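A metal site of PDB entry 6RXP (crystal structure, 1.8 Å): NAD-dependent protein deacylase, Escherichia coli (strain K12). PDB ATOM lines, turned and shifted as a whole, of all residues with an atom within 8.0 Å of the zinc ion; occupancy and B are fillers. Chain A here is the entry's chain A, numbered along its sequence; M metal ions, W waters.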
ATOM      1  N   ARG A 129      19.786  13.867 -29.511  1.00  0.00           N
ATOM      2  CA  ARG A 129      21.068  14.026 -28.867  1.00  0.00           C
ATOM      3  C   ARG A 129      21.748  15.298 -29.344  1.00  0.00           C
ATOM      4  O   ARG A 129      21.702  15.622 -30.520  1.00  0.00           O
ATOM      5  CB  ARG A 129      21.951  12.813 -29.144  1.00  0.00           C
ATOM      6  CG  ARG A 129      23.042  12.581 -28.146  1.00  0.00           C
ATOM      7  CD  ARG A 129      23.412  11.113 -28.155  1.00  0.00           C
ATOM      8  NE  ARG A 129      24.258  10.765 -29.284  1.00  0.00           N
ATOM      9  CZ  ARG A 129      24.215   9.617 -29.955  1.00  0.00           C
ATOM     10  NH1 ARG A 129      23.312   8.676 -29.659  1.00  0.00           N
ATOM     11  NH2 ARG A 129      25.055   9.420 -30.943  1.00  0.00           N
ATOM     12  N   CYS A 130      22.376  16.017 -28.426  1.00  0.00           N
ATOM     13  CA  CYS A 130      23.164  17.167 -28.830  1.00  0.00           C
ATOM     14  C   CYS A 130      24.405  16.681 -29.580  1.00  0.00           C
ATOM     15  O   CYS A 130      25.129  15.815 -29.097  1.00  0.00           O
ATOM     16  CB  CYS A 130      23.579  18.003 -27.635  1.00  0.00           C
ATOM     17  SG  CYS A 130      24.670  19.332 -28.122  1.00  0.00           S
ATOM     18  N   SER A 131      24.626  17.236 -30.763  1.00  0.00           N
ATOM     19  CA  SER A 131      25.740  16.812 -31.595  1.00  0.00           C
ATOM     20  C   SER A 131      27.075  17.232 -30.986  1.00  0.00           C
ATOM     21  O   SER A 131      28.123  16.729 -31.377  1.00  0.00           O
ATOM     22  CB  SER A 131      25.580  17.386 -33.016  1.00  0.00           C
ATOM     23  OG  SER A 131      25.496  18.806 -33.002  1.00  0.00           O
ATOM     24  N   GLN A 132      27.030  18.134 -30.013  1.00  0.00           N
ATOM     25  CA  GLN A 132      28.252  18.624 -29.383  1.00  0.00           C
ATOM     26  C   GLN A 132      28.552  17.931 -28.041  1.00  0.00           C
ATOM     27  O   GLN A 132      29.626  17.364 -27.856  1.00  0.00           O
ATOM     28  CB  GLN A 132      28.159  20.145 -29.168  1.00  0.00           C
ATOM     29  CG  GLN A 132      29.423  20.761 -28.593  1.00  0.00           C
ATOM     30  CD  GLN A 132      30.600  20.664 -29.552  1.00  0.00           C
ATOM     31  OE1 GLN A 132      31.461  19.803 -29.416  1.00  0.00           O
ATOM     32  NE2 GLN A 132      30.624  21.556 -30.535  1.00  0.00           N
ATOM     33  N   SER A 133      27.602  17.973 -27.122  1.00  0.00           N
ATOM     34  CA  SER A 133      27.824  17.407 -25.785  1.00  0.00           C
ATOM     35  C   SER A 133      27.532  15.915 -25.718  1.00  0.00           C
ATOM     36  O   SER A 133      28.020  15.216 -24.820  1.00  0.00           O
ATOM     37  CB  SER A 133      26.959  18.111 -24.745  1.00  0.00           C
ATOM     38  OG  SER A 133      25.601  17.766 -24.937  1.00  0.00           O
ATOM     39  N   GLY A 134      26.724  15.422 -26.643  1.00  0.00           N
ATOM     40  CA  GLY A 134      26.316  14.032 -26.637  1.00  0.00           C
ATOM     41  C   GLY A 134      25.211  13.743 -25.640  1.00  0.00           C
ATOM     42  O   GLY A 134      24.827  12.597 -25.450  1.00  0.00           O
ATOM     43  N   GLN A 135      24.696  14.776 -24.989  1.00  0.00           N
ATOM     44  CA  GLN A 135      23.605  14.600 -24.023  1.00  0.00           C
ATOM     45  C   GLN A 135      22.271  14.360 -24.721  1.00  0.00           C
ATOM     46  O   GLN A 135      21.944  14.994 -25.717  1.00  0.00           O
ATOM     47  CB  GLN A 135      23.509  15.816 -23.101  1.00  0.00           C
ATOM     48  CG  GLN A 135      24.696  15.928 -22.153  1.00  0.00           C
ATOM     49  CD  GLN A 135      24.497  16.988 -21.101  1.00  0.00           C
ATOM     50  OE1 GLN A 135      23.366  17.321 -20.743  1.00  0.00           O
ATOM     51  NE2 GLN A 135      25.599  17.532 -20.594  1.00  0.00           N
ATOM     52  N   LYS A 148      17.496  23.283 -31.828  1.00  0.00           N
ATOM     53  CA  LYS A 148      18.842  23.171 -31.274  1.00  0.00           C
ATOM     54  C   LYS A 148      18.817  22.680 -29.832  1.00  0.00           C
ATOM     55  O   LYS A 148      17.763  22.598 -29.212  1.00  0.00           O
ATOM     56  CB  LYS A 148      19.552  24.517 -31.355  1.00  0.00           C
ATOM     57  CG  LYS A 148      19.694  25.067 -32.778  1.00  0.00           C
ATOM     58  CD  LYS A 148      20.981  24.598 -33.423  1.00  0.00           C
ATOM     59  CE  LYS A 148      21.039  25.018 -34.885  1.00  0.00           C
ATOM     60  NZ  LYS A 148      20.627  26.426 -35.071  1.00  0.00           N
ATOM     61  N   CYS A 149      19.993  22.392 -29.281  1.00  0.00           N
ATOM     62  CA  CYS A 149      20.077  21.700 -27.996  1.00  0.00           C
ATOM     63  C   CYS A 149      19.639  22.567 -26.810  1.00  0.00           C
ATOM     64  O   CYS A 149      19.439  23.779 -26.947  1.00  0.00           O
ATOM     65  CB  CYS A 149      21.499  21.208 -27.763  1.00  0.00           C
ATOM     66  SG  CYS A 149      22.606  22.541 -27.350  1.00  0.00           S
ATOM     67  N   HIS A 150      19.515  21.925 -25.652  1.00  0.00           N
ATOM     68  CA  HIS A 150      19.138  22.609 -24.416  1.00  0.00           C
ATOM     69  C   HIS A 150      20.302  22.659 -23.435  1.00  0.00           C
ATOM     70  O   HIS A 150      20.150  23.168 -22.333  1.00  0.00           O
ATOM     71  CB  HIS A 150      17.937  21.930 -23.723  1.00  0.00           C
ATOM     72  CG  HIS A 150      16.694  21.893 -24.563  1.00  0.00           C
ATOM     73  ND1 HIS A 150      15.523  21.312 -24.111  1.00  0.00           N
ATOM     74  CD2 HIS A 150      16.442  22.348 -25.799  1.00  0.00           C
ATOM     75  CE1 HIS A 150      14.599  21.424 -25.046  1.00  0.00           C
ATOM     76  NE2 HIS A 150      15.127  22.045 -26.088  1.00  0.00           N
ATOM     77  N   CYS A 151      21.434  22.091 -23.837  1.00  0.00           N
ATOM     78  CA  CYS A 151      22.559  21.894 -22.905  1.00  0.00           C
ATOM     79  C   CYS A 151      23.714  22.868 -23.089  1.00  0.00           C
ATOM     80  O   CYS A 151      24.567  23.001 -22.206  1.00  0.00           O
ATOM     81  CB  CYS A 151      23.087  20.457 -23.005  1.00  0.00           C
ATOM     82  SG  CYS A 151      23.241  19.784 -24.685  1.00  0.00           S
ATOM     83  N   CYS A 152      23.770  23.550 -24.227  1.00  0.00           N
ATOM     84  CA  CYS A 152      24.897  24.441 -24.499  1.00  0.00           C
ATOM     85  C   CYS A 152      24.499  25.919 -24.547  1.00  0.00           C
ATOM     86  O   CYS A 152      23.400  26.256 -24.985  1.00  0.00           O
ATOM     87  CB  CYS A 152      25.559  24.049 -25.819  1.00  0.00           C
ATOM     88  SG  CYS A 152      26.223  22.386 -25.822  1.00  0.00           S
ATOM     89  N   GLN A 153      25.407  26.787 -24.111  1.00  0.00           N
ATOM     90  CA  GLN A 153      25.192  28.224 -24.186  1.00  0.00           C
ATOM     91  C   GLN A 153      24.975  28.637 -25.630  1.00  0.00           C
ATOM     92  O   GLN A 153      24.055  29.406 -25.942  1.00  0.00           O
ATOM     93  CB  GLN A 153      26.372  28.998 -23.569  1.00  0.00           C
ATOM     94  CG  GLN A 153      26.478  28.834 -22.072  1.00  0.00           C
ATOM     95  CD  GLN A 153      25.179  29.131 -21.376  1.00  0.00           C
ATOM     96  OE1 GLN A 153      24.590  28.253 -20.740  1.00  0.00           O
ATOM     97  NE2 GLN A 153      24.713  30.362 -21.485  1.00  0.00           N
ATOM     98  N   PHE A 154      25.833  28.123 -26.503  1.00  0.00           N
ATOM     99  CA  PHE A 154      25.645  28.268 -27.943  1.00  0.00           C
ATOM    100  C   PHE A 154      24.962  27.001 -28.473  1.00  0.00           C
ATOM    101  O   PHE A 154      25.613  25.972 -28.609  1.00  0.00           O
ATOM    102  CB  PHE A 154      26.972  28.497 -28.655  1.00  0.00           C
ATOM    103  CG  PHE A 154      26.866  28.471 -30.147  1.00  0.00           C
ATOM    104  CD1 PHE A 154      27.218  27.334 -30.863  1.00  0.00           C
ATOM    105  CD2 PHE A 154      26.392  29.576 -30.842  1.00  0.00           C
ATOM    106  CE1 PHE A 154      27.117  27.305 -32.244  1.00  0.00           C
ATOM    107  CE2 PHE A 154      26.279  29.544 -32.217  1.00  0.00           C
ATOM    108  CZ  PHE A 154      26.644  28.415 -32.918  1.00  0.00           C
ATOM    109  N   PRO A 155      23.658  27.096 -28.756  1.00  0.00           N
ATOM    110  CA  PRO A 155      22.822  25.942 -29.135  1.00  0.00           C
ATOM    111  C   PRO A 155      23.408  25.167 -30.326  1.00  0.00           C
ATOM    112  O   PRO A 155      23.740  25.758 -31.359  1.00  0.00           O
ATOM    113  CB  PRO A 155      21.478  26.585 -29.487  1.00  0.00           C
ATOM    114  CG  PRO A 155      21.450  27.839 -28.696  1.00  0.00           C
ATOM    115  CD  PRO A 155      22.868  28.334 -28.695  1.00  0.00           C
ATOM    116  N   ALA A 156      23.503  23.847 -30.164  1.00  0.00           N
ATOM    117  CA  ALA A 156      24.100  22.981 -31.175  1.00  0.00           C
ATOM    118  C   ALA A 156      23.032  22.167 -31.903  1.00  0.00           C
ATOM    119  O   ALA A 156      21.926  21.984 -31.379  1.00  0.00           O
ATOM    120  CB  ALA A 156      25.153  22.066 -30.526  1.00  0.00           C
ATOM    121  N   PRO A 157      23.347  21.696 -33.117  1.00  0.00           N
ATOM    122  CA  PRO A 157      22.427  20.858 -33.890  1.00  0.00           C
ATOM    123  C   PRO A 157      22.062  19.567 -33.148  1.00  0.00           C
ATOM    124  O   PRO A 157      22.850  19.075 -32.350  1.00  0.00           O
ATOM    125  CB  PRO A 157      23.226  20.537 -35.162  1.00  0.00           C
ATOM    126  CG  PRO A 157      24.149  21.680 -35.313  1.00  0.00           C
ATOM    127  CD  PRO A 157      24.540  22.070 -33.915  1.00  0.00           C
ATOM    128  N   LEU A 158      20.874  19.034 -33.430  1.00  0.00           N
ATOM    129  CA  LEU A 158      20.439  17.802 -32.802  1.00  0.00           C
ATOM    130  C   LEU A 158      20.442  16.656 -33.815  1.00  0.00           C
ATOM    131  O   LEU A 158      20.212  16.851 -35.007  1.00  0.00           O
ATOM    132  CB  LEU A 158      19.034  17.970 -32.209  1.00  0.00           C
ATOM    133  CG  LEU A 158      18.835  19.001 -31.099  1.00  0.00           C
ATOM    134  CD1 LEU A 158      17.351  19.242 -30.855  1.00  0.00           C
ATOM    135  CD2 LEU A 158      19.519  18.525 -29.822  1.00  0.00           C
HETATM  136 ZN    ZN M   1      24.288  21.092 -26.411  1.00  0.00          ZN
HETATM  137  O   HOH W   1      26.298  20.278 -26.752  1.00  0.00           O
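OG of Ser 133 sits close to SG of Cys 151, 3.1 Å away.
O of Ala 156 sits at hydrogen-bond distance from N of Cys 149 (2.9 Å).
N of Ser 133 sits close to SG of Cys 130 (3.4 Å).
The backbone NH (N) of Gln 132 sits close to the side-chain sulfur (SG) of Cys 130 (3.3 Å).
N of Cys 130 is in hydrogen-bond range of O of Gln 135 (2.9 Å).
The backbone NH of Gln 135 is in hydrogen-bond range of the side-chain hydroxyl of Ser 133, at 3.1 Å.
The zinc ion is bound by water W1 (2.2 Å), the side-chain sulfur of Cys 152 (2.4 Å), the side-chain sulfur of Cys 151 (2.4 Å), the side-chain sulfur of Cys 149 (2.4 Å) and the side-chain sulfur of Cys 130 (2.5 Å).
Ser 133 touches the zinc ion.
Five residues have an atom within 4 Å of the zinc ion: Cys 130, Ser 133, Cys 149, Cys 151 and Cys 152.
The nearest printed residue that does not touch the zinc ion is Ala 156 (4.3 Å).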
